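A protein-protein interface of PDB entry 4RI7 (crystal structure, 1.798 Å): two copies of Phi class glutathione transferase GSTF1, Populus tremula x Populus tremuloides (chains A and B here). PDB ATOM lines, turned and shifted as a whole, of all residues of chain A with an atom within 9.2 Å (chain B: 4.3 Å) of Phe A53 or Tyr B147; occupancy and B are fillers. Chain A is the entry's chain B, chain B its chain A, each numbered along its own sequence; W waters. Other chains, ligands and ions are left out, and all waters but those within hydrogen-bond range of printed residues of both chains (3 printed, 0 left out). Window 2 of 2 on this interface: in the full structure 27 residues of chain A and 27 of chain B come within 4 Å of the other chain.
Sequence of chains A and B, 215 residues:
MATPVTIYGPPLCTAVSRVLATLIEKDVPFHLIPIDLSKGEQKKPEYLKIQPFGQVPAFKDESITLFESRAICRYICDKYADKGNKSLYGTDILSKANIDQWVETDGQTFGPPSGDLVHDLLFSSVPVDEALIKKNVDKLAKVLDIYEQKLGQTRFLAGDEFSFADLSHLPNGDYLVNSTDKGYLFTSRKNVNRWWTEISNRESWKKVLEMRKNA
The side-chain hydroxyl (OG1) of Thr B109 sits at hydrogen-bond distance from the side-chain carboxylate (OE2) of Glu A68 (3.4 Å).
Water W3 lies within hydrogen-bond range of the side-chain carboxylate (OE2) of Glu A68 (2.4 Å), the side-chain hydroxyl (OG1) of Thr B109 (2.7 Å) and the side-chain hydroxyl (OG1) of Thr B105 (3.0 Å).
Water W2 bridges the backbone carbonyl oxygen of Pro A52 and the side-chain amide oxygen of Gln B149.
Water W1 lies within hydrogen-bond range of the side-chain hydroxyl (OG1) of Thr B109 (2.8 Å) and the side-chain amide oxygen (OE1) of Gln A55 (2.9 Å).
Of chain B, only Trp B102, Thr B105, Ile B146 and Tyr B147 come within 4 Å of Phe A53.
Of the printed residues of chain B, Glu A68 touches Thr B105 and Thr B109.
Printed residues of chain A within 4 Å of Thr B105: Phe A53 (3.5 Å), Phe A67 (3.3 Å) and Glu A68 (3.9 Å).
Of the printed residues of chain A, Thr B109 touches Glu A68.
Of chain A, only Pro A52 and Phe A53 come within 4 Å of Ile B146.
Of chain A, only Phe A53 (3.97 Å) comes within 4 Å of Tyr B147.
Lys B150 touches none of the printed residues of chain A.
The nearest residue of chain B that does not touch Phe A53 is Thr B109 (4.2 Å).
The nearest printed residue of chain B that does not touch Pro A52 is Trp B102 (4.7 Å).
Of the 17 printed residues of chain A, 4 touch a printed residue of chain B.
Printed residues of chain A that touch a printed residue of chain B: Pro A52, Phe A53, Phe A67 and Glu A68.
Hydrophobic or aromatic side chains of chain A that line the printed part of chain B: Phe A53 and Phe A67.
Of the 16 printed residues of chain B, 5 touch a printed residue of chain A.
Printed residues of chain B that touch a printed residue of chain A: Trp B102, Thr B105, Thr B109, Ile B146 and Tyr B147.
Among the printed residues, no Asp or Glu carboxylate lies within 4 Å of a Lys or Arg side-chain nitrogen of the other chain.
A ring nitrogen (NE2) of His B169 lies within hydrogen-bond range of the side-chain hydroxyl (OH) of Tyr B147, at 2.6 Å.
The side-chain amide oxygen (OE1) of Gln A51 sits at hydrogen-bond distance from the backbone NH (N) of Phe A53 (2.9 Å).
The side-chain amino group (NZ) of Lys A43 sits at hydrogen-bond distance from the backbone carbonyl oxygen (O) of Phe A53, at 3.4 Å.
O of Thr B105 lies within hydrogen-bond range of N of Phe B110, at 2.9 Å.
No position is printed for both chains.
Of the 9 pairs that touch across the chains among the printed residues, none has its exchanged pair printed and touching as well.
Among the printed residues, pairs that only touch across the chains: Phe A67 with Thr B105 (3.3 Å), Phe A53 with Ile B146 (3.4 Å), Phe A53 with Thr B105 (3.5 Å), Pro A52 with Ile B146 (3.5 Å), Phe A67 with Trp B102 (3.7 Å), Phe A53 with Trp B102 (3.9 Å), Glu A68 with Thr B105 (3.9 Å) and Phe A53 with Tyr B147 (3.97 Å).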
ATOM      1  N   GLN A  42      22.006   1.183  27.767  1.00  0.00           N
ATOM      2  CA  GLN A  42      21.094   2.269  27.434  1.00  0.00           C
ATOM      3  C   GLN A  42      21.805   3.481  26.847  1.00  0.00           C
ATOM      4  O   GLN A  42      21.146   4.422  26.396  1.00  0.00           O
ATOM      5  CB  GLN A  42      20.306   2.700  28.673  1.00  0.00           C
ATOM      6  CG  GLN A  42      21.065   3.579  29.676  1.00  0.00           C
ATOM      7  CD  GLN A  42      21.964   2.796  30.606  1.00  0.00           C
ATOM      8  OE1 GLN A  42      22.245   1.613  30.379  1.00  0.00           O
ATOM      9  NE2 GLN A  42      22.429   3.455  31.665  1.00  0.00           N
ATOM     10  N   LYS A  43      23.135   3.472  26.904  1.00  0.00           N
ATOM     11  CA  LYS A  43      23.944   4.559  26.350  1.00  0.00           C
ATOM     12  C   LYS A  43      24.557   4.223  25.011  1.00  0.00           C
ATOM     13  O   LYS A  43      25.261   5.043  24.431  1.00  0.00           O
ATOM     14  CB  LYS A  43      25.032   4.932  27.335  1.00  0.00           C
ATOM     15  CG  LYS A  43      24.458   5.316  28.707  1.00  0.00           C
ATOM     16  CD  LYS A  43      23.403   6.421  28.571  1.00  0.00           C
ATOM     17  CE  LYS A  43      23.133   7.136  29.900  1.00  0.00           C
ATOM     18  NZ  LYS A  43      21.875   7.935  29.908  1.00  0.00           N
ATOM     19  N   LYS A  44      24.297   3.013  24.525  1.00  0.00           N
ATOM     20  CA  LYS A  44      24.819   2.577  23.237  1.00  0.00           C
ATOM     21  C   LYS A  44      24.136   3.337  22.111  1.00  0.00           C
ATOM     22  O   LYS A  44      22.927   3.542  22.146  1.00  0.00           O
ATOM     23  CB  LYS A  44      24.623   1.076  23.051  1.00  0.00           C
ATOM     24  CG  LYS A  44      25.459   0.235  24.004  1.00  0.00           C
ATOM     25  CD  LYS A  44      25.068  -1.236  23.984  1.00  0.00           C
ATOM     26  CE  LYS A  44      25.522  -1.925  22.711  1.00  0.00           C
ATOM     27  NZ  LYS A  44      25.415  -3.399  22.846  1.00  0.00           N
ATOM     28  N   TYR A  47      20.752   2.070  20.821  1.00  0.00           N
ATOM     29  CA  TYR A  47      19.565   2.309  21.651  1.00  0.00           C
ATOM     30  C   TYR A  47      19.210   3.807  21.645  1.00  0.00           C
ATOM     31  O   TYR A  47      18.026   4.173  21.709  1.00  0.00           O
ATOM     32  CB  TYR A  47      19.764   1.811  23.088  1.00  0.00           C
ATOM     33  CG  TYR A  47      18.525   2.052  23.910  1.00  0.00           C
ATOM     34  CD1 TYR A  47      17.377   1.341  23.667  1.00  0.00           C
ATOM     35  CD2 TYR A  47      18.491   3.038  24.895  1.00  0.00           C
ATOM     36  CE1 TYR A  47      16.207   1.595  24.381  1.00  0.00           C
ATOM     37  CE2 TYR A  47      17.336   3.301  25.603  1.00  0.00           C
ATOM     38  CZ  TYR A  47      16.198   2.561  25.354  1.00  0.00           C
ATOM     39  OH  TYR A  47      15.042   2.826  26.062  1.00  0.00           O
ATOM     40  N   LEU A  48      20.214   4.683  21.527  1.00  0.00           N
ATOM     41  CA  LEU A  48      19.945   6.130  21.557  1.00  0.00           C
ATOM     42  C   LEU A  48      19.122   6.534  20.347  1.00  0.00           C
ATOM     43  O   LEU A  48      18.378   7.527  20.399  1.00  0.00           O
ATOM     44  CB  LEU A  48      21.256   6.946  21.628  1.00  0.00           C
ATOM     45  CG  LEU A  48      22.116   6.769  22.905  1.00  0.00           C
ATOM     46  CD1 LEU A  48      23.427   7.602  22.859  1.00  0.00           C
ATOM     47  CD2 LEU A  48      21.340   7.104  24.167  1.00  0.00           C
ATOM     48  N   LYS A  49      19.215   5.751  19.272  1.00  0.00           N
ATOM     49  CA  LYS A  49      18.335   5.949  18.100  1.00  0.00           C
ATOM     50  C   LYS A  49      16.853   5.808  18.458  1.00  0.00           C
ATOM     51  O   LYS A  49      15.975   6.358  17.788  1.00  0.00           O
ATOM     52  CB  LYS A  49      18.664   4.951  16.997  1.00  0.00           C
ATOM     53  CG  LYS A  49      20.053   5.132  16.383  1.00  0.00           C
ATOM     54  CD  LYS A  49      20.240   4.203  15.199  1.00  0.00           C
ATOM     55  CE  LYS A  49      21.635   4.294  14.606  1.00  0.00           C
ATOM     56  NZ  LYS A  49      21.770   3.382  13.424  1.00  0.00           N
ATOM     57  N   ILE A  50      16.597   5.034  19.505  1.00  0.00           N
ATOM     58  CA  ILE A  50      15.250   4.741  19.971  1.00  0.00           C
ATOM     59  C   ILE A  50      14.820   5.681  21.098  1.00  0.00           C
ATOM     60  O   ILE A  50      13.687   6.209  21.090  1.00  0.00           O
ATOM     61  CB  ILE A  50      15.190   3.263  20.471  1.00  0.00           C
ATOM     62  CG1 ILE A  50      15.635   2.331  19.341  1.00  0.00           C
ATOM     63  CG2 ILE A  50      13.805   2.919  21.064  1.00  0.00           C
ATOM     64  CD1 ILE A  50      15.610   0.877  19.682  1.00  0.00           C
ATOM     65  N   GLN A  51      15.712   5.855  22.081  1.00  0.00           N
ATOM     66  CA  GLN A  51      15.453   6.727  23.222  1.00  0.00           C
ATOM     67  C   GLN A  51      16.655   7.678  23.365  1.00  0.00           C
ATOM     68  O   GLN A  51      17.738   7.296  23.874  1.00  0.00           O
ATOM     69  CB  GLN A  51      15.213   5.899  24.490  1.00  0.00           C
ATOM     70  CG  GLN A  51      14.128   6.426  25.394  1.00  0.00           C
ATOM     71  CD  GLN A  51      14.572   7.596  26.244  1.00  0.00           C
ATOM     72  OE1 GLN A  51      15.649   8.171  26.048  1.00  0.00           O
ATOM     73  NE2 GLN A  51      13.736   7.962  27.199  1.00  0.00           N
ATOM     74  N   PRO A  52      16.491   8.929  22.899  1.00  0.00           N
ATOM     75  CA  PRO A  52      17.675   9.763  22.681  1.00  0.00           C
ATOM     76  C   PRO A  52      18.324  10.265  23.980  1.00  0.00           C
ATOM     77  O   PRO A  52      19.450  10.761  23.944  1.00  0.00           O
ATOM     78  CB  PRO A  52      17.123  10.918  21.839  1.00  0.00           C
ATOM     79  CG  PRO A  52      15.719  11.027  22.242  1.00  0.00           C
ATOM     80  CD  PRO A  52      15.248   9.636  22.530  1.00  0.00           C
ATOM     81  N   PHE A  53      17.624  10.114  25.104  1.00  0.00           N
ATOM     82  CA  PHE A  53      18.136  10.533  26.405  1.00  0.00           C
ATOM     83  C   PHE A  53      18.847   9.384  27.106  1.00  0.00           C
ATOM     84  O   PHE A  53      19.384   9.555  28.180  1.00  0.00           O
ATOM     85  CB  PHE A  53      17.001  11.077  27.263  1.00  0.00           C
ATOM     86  CG  PHE A  53      16.330  12.271  26.642  1.00  0.00           C
ATOM     87  CD1 PHE A  53      16.924  13.517  26.708  1.00  0.00           C
ATOM     88  CD2 PHE A  53      15.151  12.136  25.949  1.00  0.00           C
ATOM     89  CE1 PHE A  53      16.349  14.628  26.106  1.00  0.00           C
ATOM     90  CE2 PHE A  53      14.558  13.244  25.340  1.00  0.00           C
ATOM     91  CZ  PHE A  53      15.166  14.495  25.424  1.00  0.00           C
ATOM     92  N   GLY A  54      18.891   8.222  26.462  1.00  0.00           N
ATOM     93  CA  GLY A  54      19.611   7.097  27.026  1.00  0.00           C
ATOM     94  C   GLY A  54      18.960   6.577  28.298  1.00  0.00           C
ATOM     95  O   GLY A  54      19.640   6.229  29.255  1.00  0.00           O
ATOM     96  N   GLN A  55      17.626   6.537  28.293  1.00  0.00           N
ATOM     97  CA  GLN A  55      16.861   5.968  29.392  1.00  0.00           C
ATOM     98  C   GLN A  55      15.833   4.953  28.909  1.00  0.00           C
ATOM     99  O   GLN A  55      15.488   4.923  27.737  1.00  0.00           O
ATOM    100  CB  GLN A  55      16.169   7.071  30.159  1.00  0.00           C
ATOM    101  CG  GLN A  55      17.125   8.103  30.723  1.00  0.00           C
ATOM    102  CD  GLN A  55      16.447   8.973  31.760  1.00  0.00           C
ATOM    103  OE1 GLN A  55      15.415   9.607  31.494  1.00  0.00           O
ATOM    104  NE2 GLN A  55      16.999   8.982  32.959  1.00  0.00           N
ATOM    105  N   VAL A  56      15.362   4.124  29.827  1.00  0.00           N
ATOM    106  CA  VAL A  56      14.293   3.190  29.546  1.00  0.00           C
ATOM    107  C   VAL A  56      13.090   3.640  30.374  1.00  0.00           C
ATOM    108  O   VAL A  56      13.250   4.313  31.376  1.00  0.00           O
ATOM    109  CB  VAL A  56      14.679   1.728  29.890  1.00  0.00           C
ATOM    110  CG1 VAL A  56      15.737   1.203  28.913  1.00  0.00           C
ATOM    111  CG2 VAL A  56      15.194   1.614  31.306  1.00  0.00           C
ATOM    112  N   PRO A  57      11.874   3.290  29.955  1.00  0.00           N
ATOM    113  CA  PRO A  57      11.455   2.494  28.810  1.00  0.00           C
ATOM    114  C   PRO A  57      11.409   3.222  27.470  1.00  0.00           C
ATOM    115  O   PRO A  57      11.407   4.448  27.413  1.00  0.00           O
ATOM    116  CB  PRO A  57      10.025   2.100  29.188  1.00  0.00           C
ATOM    117  CG  PRO A  57       9.534   3.288  29.957  1.00  0.00           C
ATOM    118  CD  PRO A  57      10.719   3.718  30.776  1.00  0.00           C
ATOM    119  N   ALA A  58      11.318   2.434  26.409  1.00  0.00           N
ATOM    120  CA  ALA A  58      10.896   2.929  25.122  1.00  0.00           C
ATOM    121  C   ALA A  58       9.800   1.976  24.638  1.00  0.00           C
ATOM    122  O   ALA A  58       9.722   0.840  25.101  1.00  0.00           O
ATOM    123  CB  ALA A  58      12.033   2.995  24.146  1.00  0.00           C
ATOM    124  N   PHE A  67       8.786   7.449  23.744  1.00  0.00           N
ATOM    125  CA  PHE A  67       9.473   7.375  25.017  1.00  0.00           C
ATOM    126  C   PHE A  67       8.732   8.249  26.021  1.00  0.00           C
ATOM    127  O   PHE A  67       7.739   8.904  25.653  1.00  0.00           O
ATOM    128  CB  PHE A  67      10.956   7.784  24.869  1.00  0.00           C
ATOM    129  CG  PHE A  67      11.177   9.148  24.257  1.00  0.00           C
ATOM    130  CD1 PHE A  67      11.118  10.287  25.029  1.00  0.00           C
ATOM    131  CD2 PHE A  67      11.476   9.276  22.907  1.00  0.00           C
ATOM    132  CE1 PHE A  67      11.325  11.536  24.465  1.00  0.00           C
ATOM    133  CE2 PHE A  67      11.690  10.509  22.342  1.00  0.00           C
ATOM    134  CZ  PHE A  67      11.612  11.648  23.120  1.00  0.00           C
ATOM    135  N   GLU A  68       9.196   8.175  27.271  1.00  0.00           N
ATOM    136  CA  GLU A  68       8.567   8.764  28.463  1.00  0.00           C
ATOM    137  C   GLU A  68       7.343   7.947  28.883  1.00  0.00           C
ATOM    138  O   GLU A  68       6.275   7.905  28.213  1.00  0.00           O
ATOM    139  CB  GLU A  68       8.194  10.234  28.261  1.00  0.00           C
ATOM    140  CG  GLU A  68       9.346  11.206  28.440  1.00  0.00           C
ATOM    141  CD  GLU A  68       9.815  11.329  29.876  1.00  0.00           C
ATOM    142  OE1 GLU A  68       9.104  10.841  30.787  1.00  0.00           O
ATOM    143  OE2 GLU A  68      10.899  11.926  30.083  1.00  0.00           O
ATOM    144  N   TRP B 102       7.300  14.645  24.116  1.00  0.00           N
ATOM    145  CA  TRP B 102       8.153  15.818  24.329  1.00  0.00           C
ATOM    146  C   TRP B 102       7.572  16.719  25.420  1.00  0.00           C
ATOM    147  O   TRP B 102       8.307  17.437  26.113  1.00  0.00           O
ATOM    148  CB  TRP B 102       8.357  16.592  22.986  1.00  0.00           C
ATOM    149  CG  TRP B 102       9.162  15.797  22.021  1.00  0.00           C
ATOM    150  CD1 TRP B 102       8.695  15.003  21.014  1.00  0.00           C
ATOM    151  CD2 TRP B 102      10.594  15.638  22.022  1.00  0.00           C
ATOM    152  NE1 TRP B 102       9.743  14.383  20.374  1.00  0.00           N
ATOM    153  CE2 TRP B 102      10.916  14.753  20.979  1.00  0.00           C
ATOM    154  CE3 TRP B 102      11.625  16.149  22.817  1.00  0.00           C
ATOM    155  CZ2 TRP B 102      12.230  14.386  20.687  1.00  0.00           C
ATOM    156  CZ3 TRP B 102      12.937  15.790  22.524  1.00  0.00           C
ATOM    157  CH2 TRP B 102      13.228  14.918  21.466  1.00  0.00           C
ATOM    158  N   THR B 105       8.970  15.107  28.326  1.00  0.00           N
ATOM    159  CA  THR B 105      10.380  15.462  28.401  1.00  0.00           C
ATOM    160  C   THR B 105      10.519  16.815  29.095  1.00  0.00           C
ATOM    161  O   THR B 105      11.420  16.992  29.939  1.00  0.00           O
ATOM    162  CB  THR B 105      11.030  15.454  26.990  1.00  0.00           C
ATOM    163  OG1 THR B 105      11.009  14.105  26.466  1.00  0.00           O
ATOM    164  CG2 THR B 105      12.454  15.917  27.039  1.00  0.00           C
ATOM    165  N   THR B 109      12.405  15.966  32.402  1.00  0.00           N
ATOM    166  CA  THR B 109      13.811  15.983  31.999  1.00  0.00           C
ATOM    167  C   THR B 109      14.371  17.400  31.929  1.00  0.00           C
ATOM    168  O   THR B 109      15.384  17.693  32.555  1.00  0.00           O
ATOM    169  CB  THR B 109      13.979  15.265  30.650  1.00  0.00           C
ATOM    170  OG1 THR B 109      13.560  13.900  30.803  1.00  0.00           O
ATOM    171  CG2 THR B 109      15.404  15.272  30.208  1.00  0.00           C
ATOM    172  N   PHE B 110      13.700  18.264  31.181  1.00  0.00           N
ATOM    173  CA  PHE B 110      14.093  19.674  31.027  1.00  0.00           C
ATOM    174  C   PHE B 110      13.656  20.485  32.243  1.00  0.00           C
ATOM    175  O   PHE B 110      14.410  21.325  32.776  1.00  0.00           O
ATOM    176  CB  PHE B 110      13.465  20.251  29.743  1.00  0.00           C
ATOM    177  CG  PHE B 110      13.567  21.755  29.610  1.00  0.00           C
ATOM    178  CD1 PHE B 110      14.674  22.338  29.022  1.00  0.00           C
ATOM    179  CD2 PHE B 110      12.571  22.585  30.099  1.00  0.00           C
ATOM    180  CE1 PHE B 110      14.777  23.736  28.911  1.00  0.00           C
ATOM    181  CE2 PHE B 110      12.673  23.968  30.006  1.00  0.00           C
ATOM    182  CZ  PHE B 110      13.782  24.541  29.408  1.00  0.00           C
ATOM    183  N   VAL B 143      20.665  17.871  28.454  1.00  0.00           N
ATOM    184  CA  VAL B 143      19.367  17.855  27.785  1.00  0.00           C
ATOM    185  C   VAL B 143      19.409  18.685  26.497  1.00  0.00           C
ATOM    186  O   VAL B 143      18.941  18.271  25.457  1.00  0.00           O
ATOM    187  CB  VAL B 143      18.245  18.396  28.689  1.00  0.00           C
ATOM    188  CG1 VAL B 143      16.942  18.522  27.916  1.00  0.00           C
ATOM    189  CG2 VAL B 143      18.040  17.463  29.896  1.00  0.00           C
ATOM    190  N   LEU B 144      19.994  19.861  26.570  1.00  0.00           N
ATOM    191  CA  LEU B 144      20.002  20.716  25.397  1.00  0.00           C
ATOM    192  C   LEU B 144      20.926  20.222  24.301  1.00  0.00           C
ATOM    193  O   LEU B 144      20.701  20.552  23.140  1.00  0.00           O
ATOM    194  CB  LEU B 144      20.356  22.136  25.815  1.00  0.00           C
ATOM    195  CG  LEU B 144      19.269  22.754  26.714  1.00  0.00           C
ATOM    196  CD1 LEU B 144      19.696  24.114  27.230  1.00  0.00           C
ATOM    197  CD2 LEU B 144      17.977  22.895  25.925  1.00  0.00           C
ATOM    198  N   ASP B 145      21.937  19.421  24.636  1.00  0.00           N
ATOM    199  CA  ASP B 145      22.745  18.762  23.606  1.00  0.00           C
ATOM    200  C   ASP B 145      21.862  17.840  22.768  1.00  0.00           C
ATOM    201  O   ASP B 145      22.038  17.692  21.544  1.00  0.00           O
ATOM    202  CB  ASP B 145      23.884  17.924  24.210  1.00  0.00           C
ATOM    203  CG  ASP B 145      25.047  18.758  24.711  1.00  0.00           C
ATOM    204  OD1 ASP B 145      25.241  19.922  24.288  1.00  0.00           O
ATOM    205  OD2 ASP B 145      25.776  18.204  25.534  1.00  0.00           O
ATOM    206  N   ILE B 146      20.911  17.199  23.435  1.00  0.00           N
ATOM    207  CA  ILE B 146      20.017  16.303  22.738  1.00  0.00           C
ATOM    208  C   ILE B 146      19.017  17.116  21.918  1.00  0.00           C
ATOM    209  O   ILE B 146      18.770  16.802  20.742  1.00  0.00           O
ATOM    210  CB  ILE B 146      19.334  15.351  23.748  1.00  0.00           C
ATOM    211  CG1 ILE B 146      20.406  14.405  24.290  1.00  0.00           C
ATOM    212  CG2 ILE B 146      18.222  14.578  23.088  1.00  0.00           C
ATOM    213  CD1 ILE B 146      20.099  13.800  25.614  1.00  0.00           C
ATOM    214  N   TYR B 147      18.474  18.184  22.505  1.00  0.00           N
ATOM    215  CA  TYR B 147      17.646  19.120  21.735  1.00  0.00           C
ATOM    216  C   TYR B 147      18.351  19.664  20.496  1.00  0.00           C
ATOM    217  O   TYR B 147      17.717  19.843  19.433  1.00  0.00           O
ATOM    218  CB  TYR B 147      17.220  20.293  22.601  1.00  0.00           C
ATOM    219  CG  TYR B 147      16.157  19.995  23.644  1.00  0.00           C
ATOM    220  CD1 TYR B 147      15.892  18.691  24.068  1.00  0.00           C
ATOM    221  CD2 TYR B 147      15.425  21.030  24.215  1.00  0.00           C
ATOM    222  CE1 TYR B 147      14.914  18.434  25.046  1.00  0.00           C
ATOM    223  CE2 TYR B 147      14.446  20.785  25.164  1.00  0.00           C
ATOM    224  CZ  TYR B 147      14.204  19.475  25.589  1.00  0.00           C
ATOM    225  OH  TYR B 147      13.234  19.247  26.552  1.00  0.00           O
ATOM    226  N   GLU B 148      19.637  19.974  20.631  1.00  0.00           N
ATOM    227  CA  GLU B 148      20.392  20.545  19.530  1.00  0.00           C
ATOM    228  C   GLU B 148      20.371  19.585  18.343  1.00  0.00           C
ATOM    229  O   GLU B 148      20.191  20.009  17.210  1.00  0.00           O
ATOM    230  CB  GLU B 148      21.828  20.846  19.940  1.00  0.00           C
ATOM    231  CG  GLU B 148      22.698  21.431  18.865  1.00  0.00           C
ATOM    232  CD  GLU B 148      22.246  22.807  18.377  1.00  0.00           C
ATOM    233  OE1 GLU B 148      21.387  23.437  19.042  1.00  0.00           O
ATOM    234  OE2 GLU B 148      22.748  23.235  17.312  1.00  0.00           O
ATOM    235  N   GLN B 149      20.590  18.300  18.602  1.00  0.00           N
ATOM    236  CA  GLN B 149      20.568  17.300  17.548  1.00  0.00           C
ATOM    237  C   GLN B 149      19.167  17.209  16.929  1.00  0.00           C
ATOM    238  O   GLN B 149      19.010  17.179  15.698  1.00  0.00           O
ATOM    239  CB  GLN B 149      20.983  15.920  18.086  1.00  0.00           C
ATOM    240  CG  GLN B 149      22.365  15.833  18.737  1.00  0.00           C
ATOM    241  CD  GLN B 149      22.508  14.593  19.632  1.00  0.00           C
ATOM    242  OE1 GLN B 149      21.761  13.614  19.485  1.00  0.00           O
ATOM    243  NE2 GLN B 149      23.451  14.642  20.574  1.00  0.00           N
ATOM    244  N   LYS B 150      18.149  17.175  17.783  1.00  0.00           N
ATOM    245  CA  LYS B 150      16.777  16.993  17.325  1.00  0.00           C
ATOM    246  C   LYS B 150      16.336  18.172  16.472  1.00  0.00           C
ATOM    247  O   LYS B 150      15.647  17.996  15.463  1.00  0.00           O
ATOM    248  CB  LYS B 150      15.832  16.834  18.518  1.00  0.00           C
ATOM    249  CG  LYS B 150      14.377  16.514  18.151  1.00  0.00           C
ATOM    250  CD  LYS B 150      14.221  15.154  17.456  1.00  0.00           C
ATOM    251  CE  LYS B 150      12.754  14.792  17.203  1.00  0.00           C
ATOM    252  NZ  LYS B 150      12.102  15.677  16.225  1.00  0.00           N
ATOM    253  N   LEU B 151      16.746  19.366  16.895  1.00  0.00           N
ATOM    254  CA  LEU B 151      16.317  20.608  16.258  1.00  0.00           C
ATOM    255  C   LEU B 151      17.119  20.893  14.966  1.00  0.00           C
ATOM    256  O   LEU B 151      16.820  21.837  14.226  1.00  0.00           O
ATOM    257  CB  LEU B 151      16.441  21.761  17.257  1.00  0.00           C
ATOM    258  CG  LEU B 151      15.377  21.695  18.375  1.00  0.00           C
ATOM    259  CD1 LEU B 151      15.695  22.680  19.496  1.00  0.00           C
ATOM    260  CD2 LEU B 151      13.968  21.947  17.810  1.00  0.00           C
ATOM    261  N   LEU B 157      10.369  20.679  18.442  1.00  0.00           N
ATOM    262  CA  LEU B 157      10.779  19.450  19.110  1.00  0.00           C
ATOM    263  C   LEU B 157      10.105  18.194  18.528  1.00  0.00           C
ATOM    264  O   LEU B 157      10.750  17.173  18.326  1.00  0.00           O
ATOM    265  CB  LEU B 157      10.490  19.554  20.609  1.00  0.00           C
ATOM    266  CG  LEU B 157      11.433  20.453  21.417  1.00  0.00           C
ATOM    267  CD1 LEU B 157      10.920  20.658  22.830  1.00  0.00           C
ATOM    268  CD2 LEU B 157      12.825  19.882  21.482  1.00  0.00           C
ATOM    269  N   HIS B 169       8.038  24.616  27.253  1.00  0.00           N
ATOM    270  CA  HIS B 169       9.385  25.070  27.578  1.00  0.00           C
ATOM    271  C   HIS B 169       9.527  26.584  27.758  1.00  0.00           C
ATOM    272  O   HIS B 169      10.575  27.065  28.221  1.00  0.00           O
ATOM    273  CB  HIS B 169      10.354  24.632  26.477  1.00  0.00           C
ATOM    274  CG  HIS B 169      10.623  23.167  26.455  1.00  0.00           C
ATOM    275  ND1 HIS B 169       9.717  22.242  25.967  1.00  0.00           N
ATOM    276  CD2 HIS B 169      11.697  22.460  26.883  1.00  0.00           C
ATOM    277  CE1 HIS B 169      10.235  21.031  26.084  1.00  0.00           C
ATOM    278  NE2 HIS B 169      11.436  21.137  26.630  1.00  0.00           N
ATOM    279  N   VAL B 192      19.067  25.186  18.906  1.00  0.00           N
ATOM    280  CA  VAL B 192      18.266  25.538  20.066  1.00  0.00           C
ATOM    281  C   VAL B 192      18.025  27.041  20.081  1.00  0.00           C
ATOM    282  O   VAL B 192      16.949  27.499  20.445  1.00  0.00           O
ATOM    283  CB  VAL B 192      18.945  25.123  21.378  1.00  0.00           C
ATOM    284  CG1 VAL B 192      18.249  25.784  22.579  1.00  0.00           C
ATOM    285  CG2 VAL B 192      18.935  23.590  21.512  1.00  0.00           C
HETATM  286  O   HOH W   1      13.582  11.653  32.417  1.00  0.00           O
HETATM  287  O   HOH W   2      20.808  10.978  21.555  1.00  0.00           O
HETATM  288  O   HOH W   3      12.644  12.679  28.547  1.00  0.00           O
